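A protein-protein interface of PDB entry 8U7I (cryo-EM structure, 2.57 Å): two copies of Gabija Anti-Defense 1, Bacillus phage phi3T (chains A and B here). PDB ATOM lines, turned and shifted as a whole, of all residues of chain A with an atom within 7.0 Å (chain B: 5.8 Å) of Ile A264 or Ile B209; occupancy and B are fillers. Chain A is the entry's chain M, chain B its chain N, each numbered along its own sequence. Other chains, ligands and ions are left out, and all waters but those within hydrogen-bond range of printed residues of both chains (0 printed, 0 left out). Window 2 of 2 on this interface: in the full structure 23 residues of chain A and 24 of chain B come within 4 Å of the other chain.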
ATOM      1  N   LEU A 162      -6.792   2.925   4.011  1.00  0.00           N
ATOM      2  CA  LEU A 162      -8.033   3.585   4.391  1.00  0.00           C
ATOM      3  C   LEU A 162      -9.138   3.239   3.402  1.00  0.00           C
ATOM      4  O   LEU A 162      -8.917   3.197   2.188  1.00  0.00           O
ATOM      5  CB  LEU A 162      -7.834   5.098   4.453  1.00  0.00           C
ATOM      6  CG  LEU A 162      -7.784   5.718   5.851  1.00  0.00           C
ATOM      7  CD1 LEU A 162      -8.177   7.184   5.801  1.00  0.00           C
ATOM      8  CD2 LEU A 162      -8.671   4.953   6.821  1.00  0.00           C
ATOM      9  N   ILE A 170     -12.459  12.802   5.019  1.00  0.00           N
ATOM     10  CA  ILE A 170     -11.455  13.737   5.512  1.00  0.00           C
ATOM     11  C   ILE A 170     -11.001  14.707   4.424  1.00  0.00           C
ATOM     12  O   ILE A 170     -10.511  15.797   4.737  1.00  0.00           O
ATOM     13  CB  ILE A 170     -10.270  12.995   6.167  1.00  0.00           C
ATOM     14  CG1 ILE A 170      -9.873  11.707   5.431  1.00  0.00           C
ATOM     15  CG2 ILE A 170     -10.585  12.678   7.620  1.00  0.00           C
ATOM     16  CD1 ILE A 170      -9.405  11.871   4.015  1.00  0.00           C
ATOM     17  N   ILE A 171     -11.149  14.352   3.146  1.00  0.00           N
ATOM     18  CA  ILE A 171     -10.862  15.331   2.103  1.00  0.00           C
ATOM     19  C   ILE A 171     -11.944  16.401   2.076  1.00  0.00           C
ATOM     20  O   ILE A 171     -11.655  17.588   1.886  1.00  0.00           O
ATOM     21  CB  ILE A 171     -10.688  14.654   0.730  1.00  0.00           C
ATOM     22  CG1 ILE A 171     -11.971  13.959   0.279  1.00  0.00           C
ATOM     23  CG2 ILE A 171      -9.538  13.662   0.773  1.00  0.00           C
ATOM     24  CD1 ILE A 171     -11.741  12.890  -0.760  1.00  0.00           C
ATOM     25  N   GLU A 250     -10.703   7.714  -4.624  1.00  0.00           N
ATOM     26  CA  GLU A 250      -9.721   6.644  -4.479  1.00  0.00           C
ATOM     27  C   GLU A 250      -9.430   6.410  -3.002  1.00  0.00           C
ATOM     28  O   GLU A 250      -9.238   7.376  -2.253  1.00  0.00           O
ATOM     29  CB  GLU A 250      -8.462   6.975  -5.299  1.00  0.00           C
ATOM     30  CG  GLU A 250      -7.436   8.058  -4.842  1.00  0.00           C
ATOM     31  CD  GLU A 250      -6.693   7.821  -3.532  1.00  0.00           C
ATOM     32  OE1 GLU A 250      -6.746   6.712  -2.970  1.00  0.00           O
ATOM     33  OE2 GLU A 250      -6.039   8.774  -3.060  1.00  0.00           O
ATOM     34  N   PHE A 252      -7.325   5.787   0.136  1.00  0.00           N
ATOM     35  CA  PHE A 252      -5.913   5.991   0.428  1.00  0.00           C
ATOM     36  C   PHE A 252      -5.273   4.703   0.926  1.00  0.00           C
ATOM     37  O   PHE A 252      -5.821   4.006   1.785  1.00  0.00           O
ATOM     38  CB  PHE A 252      -5.741   7.097   1.466  1.00  0.00           C
ATOM     39  CG  PHE A 252      -6.245   8.435   1.016  1.00  0.00           C
ATOM     40  CD1 PHE A 252      -5.552   9.171   0.072  1.00  0.00           C
ATOM     41  CD2 PHE A 252      -7.395   8.974   1.565  1.00  0.00           C
ATOM     42  CE1 PHE A 252      -6.011  10.408  -0.334  1.00  0.00           C
ATOM     43  CE2 PHE A 252      -7.857  10.210   1.164  1.00  0.00           C
ATOM     44  CZ  PHE A 252      -7.164  10.929   0.214  1.00  0.00           C
ATOM     45  N   SER A 253      -4.102   4.388   0.379  1.00  0.00           N
ATOM     46  CA  SER A 253      -3.359   3.188   0.735  1.00  0.00           C
ATOM     47  C   SER A 253      -1.969   3.583   1.205  1.00  0.00           C
ATOM     48  O   SER A 253      -1.273   4.347   0.528  1.00  0.00           O
ATOM     49  CB  SER A 253      -3.265   2.227  -0.452  1.00  0.00           C
ATOM     50  OG  SER A 253      -2.762   2.888  -1.600  1.00  0.00           O
ATOM     51  N   GLY A 254      -1.570   3.067   2.364  1.00  0.00           N
ATOM     52  CA  GLY A 254      -0.260   3.356   2.907  1.00  0.00           C
ATOM     53  C   GLY A 254       0.367   2.163   3.596  1.00  0.00           C
ATOM     54  O   GLY A 254      -0.297   1.464   4.368  1.00  0.00           O
ATOM     55  N   VAL A 257       1.487   3.796   8.888  1.00  0.00           N
ATOM     56  CA  VAL A 257       0.528   4.820   9.299  1.00  0.00           C
ATOM     57  C   VAL A 257       1.095   6.212   9.052  1.00  0.00           C
ATOM     58  O   VAL A 257       0.423   7.085   8.490  1.00  0.00           O
ATOM     59  CB  VAL A 257       0.131   4.621  10.773  1.00  0.00           C
ATOM     60  CG1 VAL A 257      -0.394   5.919  11.368  1.00  0.00           C
ATOM     61  CG2 VAL A 257      -0.905   3.514  10.898  1.00  0.00           C
ATOM     62  N   GLU A 258       2.344   6.439   9.457  1.00  0.00           N
ATOM     63  CA  GLU A 258       2.998   7.702   9.144  1.00  0.00           C
ATOM     64  C   GLU A 258       3.246   7.859   7.651  1.00  0.00           C
ATOM     65  O   GLU A 258       3.148   8.976   7.132  1.00  0.00           O
ATOM     66  CB  GLU A 258       4.326   7.817   9.898  1.00  0.00           C
ATOM     67  CG  GLU A 258       4.200   8.089  11.395  1.00  0.00           C
ATOM     68  CD  GLU A 258       2.851   8.653  11.799  1.00  0.00           C
ATOM     69  OE1 GLU A 258       2.148   7.992  12.592  1.00  0.00           O
ATOM     70  OE2 GLU A 258       2.504   9.770  11.356  1.00  0.00           O
ATOM     71  N   ASP A 259       3.569   6.765   6.958  1.00  0.00           N
ATOM     72  CA  ASP A 259       3.717   6.814   5.508  1.00  0.00           C
ATOM     73  C   ASP A 259       2.397   7.203   4.856  1.00  0.00           C
ATOM     74  O   ASP A 259       2.360   8.038   3.944  1.00  0.00           O
ATOM     75  CB  ASP A 259       4.217   5.452   5.009  1.00  0.00           C
ATOM     76  CG  ASP A 259       3.796   5.132   3.576  1.00  0.00           C
ATOM     77  OD1 ASP A 259       3.687   6.044   2.730  1.00  0.00           O
ATOM     78  OD2 ASP A 259       3.564   3.937   3.296  1.00  0.00           O
ATOM     79  N   LEU A 260       1.294   6.616   5.326  1.00  0.00           N
ATOM     80  CA  LEU A 260      -0.016   6.970   4.791  1.00  0.00           C
ATOM     81  C   LEU A 260      -0.342   8.433   5.053  1.00  0.00           C
ATOM     82  O   LEU A 260      -0.847   9.130   4.164  1.00  0.00           O
ATOM     83  CB  LEU A 260      -1.093   6.068   5.389  1.00  0.00           C
ATOM     84  CG  LEU A 260      -2.489   6.238   4.787  1.00  0.00           C
ATOM     85  CD1 LEU A 260      -2.415   6.265   3.272  1.00  0.00           C
ATOM     86  CD2 LEU A 260      -3.426   5.140   5.259  1.00  0.00           C
ATOM     87  N   LYS A 261      -0.054   8.921   6.263  1.00  0.00           N
ATOM     88  CA  LYS A 261      -0.360  10.312   6.581  1.00  0.00           C
ATOM     89  C   LYS A 261       0.376  11.257   5.643  1.00  0.00           C
ATOM     90  O   LYS A 261      -0.204  12.225   5.140  1.00  0.00           O
ATOM     91  CB  LYS A 261      -0.004  10.622   8.034  1.00  0.00           C
ATOM     92  CG  LYS A 261      -0.530  11.975   8.490  1.00  0.00           C
ATOM     93  CD  LYS A 261      -0.454  12.150   9.996  1.00  0.00           C
ATOM     94  CE  LYS A 261       0.974  12.397  10.452  1.00  0.00           C
ATOM     95  NZ  LYS A 261       1.038  12.792  11.886  1.00  0.00           N
ATOM     96  N   SER A 262       1.656  10.984   5.389  1.00  0.00           N
ATOM     97  CA  SER A 262       2.405  11.790   4.431  1.00  0.00           C
ATOM     98  C   SER A 262       1.812  11.672   3.032  1.00  0.00           C
ATOM     99  O   SER A 262       1.721  12.668   2.304  1.00  0.00           O
ATOM    100  CB  SER A 262       3.872  11.369   4.426  1.00  0.00           C
ATOM    101  OG  SER A 262       4.081  10.278   3.547  1.00  0.00           O
ATOM    102  N   ASN A 263       1.407  10.463   2.641  1.00  0.00           N
ATOM    103  CA  ASN A 263       0.840  10.265   1.313  1.00  0.00           C
ATOM    104  C   ASN A 263      -0.440  11.071   1.134  1.00  0.00           C
ATOM    105  O   ASN A 263      -0.623  11.751   0.118  1.00  0.00           O
ATOM    106  CB  ASN A 263       0.577   8.780   1.072  1.00  0.00           C
ATOM    107  CG  ASN A 263       0.626   8.412  -0.394  1.00  0.00           C
ATOM    108  OD1 ASN A 263       1.361   9.018  -1.172  1.00  0.00           O
ATOM    109  ND2 ASN A 263      -0.157   7.412  -0.781  1.00  0.00           N
ATOM    110  N   ILE A 264      -1.340  11.011   2.116  1.00  0.00           N
ATOM    111  CA  ILE A 264      -2.594  11.744   1.984  1.00  0.00           C
ATOM    112  C   ILE A 264      -2.361  13.230   2.212  1.00  0.00           C
ATOM    113  O   ILE A 264      -3.083  14.071   1.662  1.00  0.00           O
ATOM    114  CB  ILE A 264      -3.663  11.174   2.938  1.00  0.00           C
ATOM    115  CG1 ILE A 264      -3.376  11.552   4.385  1.00  0.00           C
ATOM    116  CG2 ILE A 264      -3.683   9.670   2.858  1.00  0.00           C
ATOM    117  CD1 ILE A 264      -4.239  12.685   4.860  1.00  0.00           C
ATOM    118  N   LYS A 265      -1.361  13.581   3.027  1.00  0.00           N
ATOM    119  CA  LYS A 265      -1.047  14.989   3.242  1.00  0.00           C
ATOM    120  C   LYS A 265      -0.644  15.661   1.939  1.00  0.00           C
ATOM    121  O   LYS A 265      -1.204  16.697   1.565  1.00  0.00           O
ATOM    122  CB  LYS A 265       0.068  15.139   4.275  1.00  0.00           C
ATOM    123  CG  LYS A 265       0.556  16.570   4.435  1.00  0.00           C
ATOM    124  CD  LYS A 265       1.717  16.663   5.407  1.00  0.00           C
ATOM    125  CE  LYS A 265       2.109  18.112   5.648  1.00  0.00           C
ATOM    126  NZ  LYS A 265       1.067  18.854   6.408  1.00  0.00           N
ATOM    127  N   LYS A 266       0.320  15.076   1.227  1.00  0.00           N
ATOM    128  CA  LYS A 266       0.745  15.667  -0.034  1.00  0.00           C
ATOM    129  C   LYS A 266      -0.377  15.645  -1.062  1.00  0.00           C
ATOM    130  O   LYS A 266      -0.424  16.512  -1.939  1.00  0.00           O
ATOM    131  CB  LYS A 266       1.978  14.948  -0.580  1.00  0.00           C
ATOM    132  CG  LYS A 266       1.698  13.587  -1.191  1.00  0.00           C
ATOM    133  CD  LYS A 266       2.891  13.085  -1.985  1.00  0.00           C
ATOM    134  CE  LYS A 266       2.650  11.683  -2.520  1.00  0.00           C
ATOM    135  NZ  LYS A 266       1.451  11.617  -3.405  1.00  0.00           N
ATOM    136  N   PHE A 267      -1.286  14.670  -0.968  1.00  0.00           N
ATOM    137  CA  PHE A 267      -2.429  14.624  -1.873  1.00  0.00           C
ATOM    138  C   PHE A 267      -3.373  15.792  -1.624  1.00  0.00           C
ATOM    139  O   PHE A 267      -3.983  16.324  -2.558  1.00  0.00           O
ATOM    140  CB  PHE A 267      -3.170  13.296  -1.720  1.00  0.00           C
ATOM    141  CG  PHE A 267      -4.476  13.243  -2.460  1.00  0.00           C
ATOM    142  CD1 PHE A 267      -4.507  12.959  -3.813  1.00  0.00           C
ATOM    143  CD2 PHE A 267      -5.673  13.470  -1.802  1.00  0.00           C
ATOM    144  CE1 PHE A 267      -5.705  12.907  -4.498  1.00  0.00           C
ATOM    145  CE2 PHE A 267      -6.874  13.418  -2.481  1.00  0.00           C
ATOM    146  CZ  PHE A 267      -6.890  13.136  -3.830  1.00  0.00           C
ATOM    147  N   LEU A 268      -3.534  16.182  -0.360  1.00  0.00           N
ATOM    148  CA  LEU A 268      -4.415  17.301  -0.049  1.00  0.00           C
ATOM    149  C   LEU A 268      -3.841  18.617  -0.560  1.00  0.00           C
ATOM    150  O   LEU A 268      -4.576  19.451  -1.097  1.00  0.00           O
ATOM    151  CB  LEU A 268      -4.663  17.365   1.456  1.00  0.00           C
ATOM    152  CG  LEU A 268      -5.540  16.238   2.001  1.00  0.00           C
ATOM    153  CD1 LEU A 268      -6.061  16.578   3.383  1.00  0.00           C
ATOM    154  CD2 LEU A 268      -6.690  15.951   1.051  1.00  0.00           C
ATOM    155  N   ASP A 269      -2.531  18.821  -0.405  1.00  0.00           N
ATOM    156  CA  ASP A 269      -1.947  20.120  -0.727  1.00  0.00           C
ATOM    157  C   ASP A 269      -2.002  20.415  -2.223  1.00  0.00           C
ATOM    158  O   ASP A 269      -2.477  21.479  -2.632  1.00  0.00           O
ATOM    159  CB  ASP A 269      -0.510  20.196  -0.213  1.00  0.00           C
ATOM    160  CG  ASP A 269      -0.329  19.482   1.106  1.00  0.00           C
ATOM    161  OD1 ASP A 269       0.673  18.752   1.261  1.00  0.00           O
ATOM    162  OD2 ASP A 269      -1.198  19.644   1.989  1.00  0.00           O
ATOM    163  N   ASP A 270      -1.525  19.487  -3.059  1.00  0.00           N
ATOM    164  CA  ASP A 270      -1.474  19.778  -4.492  1.00  0.00           C
ATOM    165  C   ASP A 270      -2.877  19.906  -5.064  1.00  0.00           C
ATOM    166  O   ASP A 270      -3.132  20.760  -5.921  1.00  0.00           O
ATOM    167  CB  ASP A 270      -0.692  18.699  -5.242  1.00  0.00           C
ATOM    168  CG  ASP A 270      -1.295  17.323  -5.081  1.00  0.00           C
ATOM    169  OD1 ASP A 270      -1.888  17.059  -4.021  1.00  0.00           O
ATOM    170  OD2 ASP A 270      -1.177  16.504  -6.016  1.00  0.00           O
ATOM    171  N   TYR B 203      -7.254  24.679  15.101  1.00  0.00           N
ATOM    172  CA  TYR B 203      -6.510  24.955  13.876  1.00  0.00           C
ATOM    173  C   TYR B 203      -7.042  24.168  12.683  1.00  0.00           C
ATOM    174  O   TYR B 203      -7.363  22.983  12.790  1.00  0.00           O
ATOM    175  CB  TYR B 203      -5.026  24.653  14.146  1.00  0.00           C
ATOM    176  CG  TYR B 203      -4.560  23.231  13.870  1.00  0.00           C
ATOM    177  CD1 TYR B 203      -4.272  22.376  14.927  1.00  0.00           C
ATOM    178  CD2 TYR B 203      -4.333  22.765  12.582  1.00  0.00           C
ATOM    179  CE1 TYR B 203      -3.834  21.086  14.709  1.00  0.00           C
ATOM    180  CE2 TYR B 203      -3.899  21.476  12.359  1.00  0.00           C
ATOM    181  CZ  TYR B 203      -3.645  20.644  13.422  1.00  0.00           C
ATOM    182  OH  TYR B 203      -3.201  19.360  13.195  1.00  0.00           O
ATOM    183  N   HIS B 206      -4.878  20.461   8.165  1.00  0.00           N
ATOM    184  CA  HIS B 206      -4.497  19.118   8.602  1.00  0.00           C
ATOM    185  C   HIS B 206      -4.762  18.937  10.101  1.00  0.00           C
ATOM    186  O   HIS B 206      -3.853  18.819  10.920  1.00  0.00           O
ATOM    187  CB  HIS B 206      -3.036  18.806   8.257  1.00  0.00           C
ATOM    188  CG  HIS B 206      -2.817  18.456   6.820  1.00  0.00           C
ATOM    189  ND1 HIS B 206      -2.569  19.404   5.851  1.00  0.00           N
ATOM    190  CD2 HIS B 206      -2.824  17.260   6.184  1.00  0.00           C
ATOM    191  CE1 HIS B 206      -2.423  18.807   4.681  1.00  0.00           C
ATOM    192  NE2 HIS B 206      -2.575  17.507   4.856  1.00  0.00           N
ATOM    193  N   GLU B 207      -6.051  18.959  10.437  1.00  0.00           N
ATOM    194  CA  GLU B 207      -6.469  18.637  11.797  1.00  0.00           C
ATOM    195  C   GLU B 207      -6.855  17.174  11.958  1.00  0.00           C
ATOM    196  O   GLU B 207      -6.442  16.530  12.929  1.00  0.00           O
ATOM    197  CB  GLU B 207      -7.640  19.522  12.228  1.00  0.00           C
ATOM    198  CG  GLU B 207      -7.950  19.404  13.714  1.00  0.00           C
ATOM    199  CD  GLU B 207      -8.224  20.737  14.370  1.00  0.00           C
ATOM    200  OE1 GLU B 207      -9.317  21.306  14.156  1.00  0.00           O
ATOM    201  OE2 GLU B 207      -7.331  21.226  15.091  1.00  0.00           O
ATOM    202  N   TYR B 208      -7.643  16.633  11.027  1.00  0.00           N
ATOM    203  CA  TYR B 208      -8.123  15.263  11.154  1.00  0.00           C
ATOM    204  C   TYR B 208      -7.027  14.216  11.003  1.00  0.00           C
ATOM    205  O   TYR B 208      -7.279  13.045  11.306  1.00  0.00           O
ATOM    206  CB  TYR B 208      -9.235  14.993  10.135  1.00  0.00           C
ATOM    207  CG  TYR B 208     -10.608  15.469  10.567  1.00  0.00           C
ATOM    208  CD1 TYR B 208     -11.360  14.728  11.472  1.00  0.00           C
ATOM    209  CD2 TYR B 208     -11.158  16.642  10.066  1.00  0.00           C
ATOM    210  CE1 TYR B 208     -12.615  15.144  11.876  1.00  0.00           C
ATOM    211  CE2 TYR B 208     -12.420  17.068  10.467  1.00  0.00           C
ATOM    212  CZ  TYR B 208     -13.141  16.312  11.370  1.00  0.00           C
ATOM    213  OH  TYR B 208     -14.391  16.719  11.777  1.00  0.00           O
ATOM    214  N   ILE B 209      -5.833  14.587  10.542  1.00  0.00           N
ATOM    215  CA  ILE B 209      -4.787  13.581  10.383  1.00  0.00           C
ATOM    216  C   ILE B 209      -4.273  13.109  11.741  1.00  0.00           C
ATOM    217  O   ILE B 209      -3.741  11.999  11.864  1.00  0.00           O
ATOM    218  CB  ILE B 209      -3.663  14.098   9.462  1.00  0.00           C
ATOM    219  CG1 ILE B 209      -3.348  15.583   9.661  1.00  0.00           C
ATOM    220  CG2 ILE B 209      -4.046  13.883   8.027  1.00  0.00           C
ATOM    221  CD1 ILE B 209      -2.813  15.961  11.004  1.00  0.00           C
ATOM    222  N   VAL B 210      -4.413  13.940  12.779  1.00  0.00           N
ATOM    223  CA  VAL B 210      -4.047  13.495  14.120  1.00  0.00           C
ATOM    224  C   VAL B 210      -5.003  12.412  14.603  1.00  0.00           C
ATOM    225  O   VAL B 210      -4.630  11.562  15.421  1.00  0.00           O
ATOM    226  CB  VAL B 210      -3.998  14.688  15.099  1.00  0.00           C
ATOM    227  CG1 VAL B 210      -3.513  15.941  14.395  1.00  0.00           C
ATOM    228  CG2 VAL B 210      -5.358  14.928  15.751  1.00  0.00           C
ATOM    229  N   ASP B 211      -6.243  12.421  14.111  1.00  0.00           N
ATOM    230  CA  ASP B 211      -7.218  11.422  14.531  1.00  0.00           C
ATOM    231  C   ASP B 211      -6.916  10.080  13.875  1.00  0.00           C
ATOM    232  O   ASP B 211      -6.922   9.039  14.545  1.00  0.00           O
ATOM    233  CB  ASP B 211      -8.623  11.947  14.193  1.00  0.00           C
ATOM    234  CG  ASP B 211      -9.733  10.892  14.272  1.00  0.00           C
ATOM    235  OD1 ASP B 211     -10.904  11.308  14.136  1.00  0.00           O
ATOM    236  OD2 ASP B 211      -9.494   9.690  14.499  1.00  0.00           O
ATOM    237  N   LEU B 212      -6.605  10.091  12.576  1.00  0.00           N
ATOM    238  CA  LEU B 212      -6.396   8.845  11.847  1.00  0.00           C
ATOM    239  C   LEU B 212      -5.159   8.106  12.345  1.00  0.00           C
ATOM    240  O   LEU B 212      -5.168   6.874  12.448  1.00  0.00           O
ATOM    241  CB  LEU B 212      -6.315   9.130  10.341  1.00  0.00           C
ATOM    242  CG  LEU B 212      -5.068   9.651   9.604  1.00  0.00           C
ATOM    243  CD1 LEU B 212      -3.996   8.584   9.368  1.00  0.00           C
ATOM    244  CD2 LEU B 212      -5.459  10.312   8.284  1.00  0.00           C
ATOM    245  N   ASN B 213      -4.085   8.835  12.652  1.00  0.00           N
ATOM    246  CA  ASN B 213      -2.870   8.177  13.117  1.00  0.00           C
ATOM    247  C   ASN B 213      -2.991   7.697  14.556  1.00  0.00           C
ATOM    248  O   ASN B 213      -2.181   6.871  14.991  1.00  0.00           O
ATOM    249  CB  ASN B 213      -1.662   9.110  12.951  1.00  0.00           C
ATOM    250  CG  ASN B 213      -1.781  10.396  13.758  1.00  0.00           C
ATOM    251  OD1 ASN B 213      -2.163  10.385  14.928  1.00  0.00           O
ATOM    252  ND2 ASN B 213      -1.450  11.517  13.128  1.00  0.00           N
ATOM    253  N   ALA B 214      -3.979   8.198  15.301  1.00  0.00           N
ATOM    254  CA  ALA B 214      -4.161   7.770  16.684  1.00  0.00           C
ATOM    255  C   ALA B 214      -4.514   6.290  16.766  1.00  0.00           C
ATOM    256  O   ALA B 214      -4.012   5.574  17.641  1.00  0.00           O
ATOM    257  CB  ALA B 214      -5.239   8.619  17.358  1.00  0.00           C
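The side-chain amide nitrogen (ND2) of Asn B213 lies close to the side-chain amino group (NZ) of Lys A261 (3.1 Å).
The side-chain carboxylate (OE2) of Glu A258 is in salt-bridge range of the side-chain amino group (NZ) of Lys A261, at 3.4 Å. O of His B206 is in hydrogen-bond range of OH of Tyr B203. O of Ile B209 sits at hydrogen-bond distance from ND2 of Asn B213. The side-chain amide oxygen (OD1) of Asn B213 lies close to the backbone carbonyl oxygen (O) of Val B210 (2.8 Å).
CB of Tyr B208 touches CG2 of Ile A170, 3.7 Å away. Asn B213 touches Val A257 (CA to CG1, 3.8 Å). OE1 of Glu A258 touches CB of Asn B213, at 3.99 Å. Ile B209 touches Lys A261 (O to CD, 3.8 Å). Ile B209 touches Ile A264 (CG2 to CD1, 3.4 Å). His B206 touches Lys A265 (NE2 to CG, 3.3 Å). NE2 of His B206 touches CD1 of Leu A268, 3.9 Å away. OD2 of Asp A269 touches CE1 of His B206 (3.1 Å).
Ile A264 touches one residue of chain B. Of the printed residues of chain B, Leu A268 touches His B206 (3.9 Å). Of the printed residues of chain A, His B206 touches Lys A265, Leu A268 and Asp A269. Of the printed residues of chain B, Lys A261 touches Ile B209 and Asn B213. Printed residues of chain A within 4 Å of Tyr B208: Ile A170 (3.7 Å). The nearest residue of chain A that does not touch Ile B209 is Lys A265 (5.7 Å).
Of the 10 printed residues of chain B, 4 touch a printed residue of chain A. Hydrophobic or aromatic side chains of chain B within 4 Å of the printed part of chain A: His B206, Tyr B208 and Ile B209. Among the printed residues, 9 pairs touch across the chains.
No position is printed for both chains. Of the 9 pairs that touch across the chains among the printed residues, none has its exchanged pair printed and touching as well.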
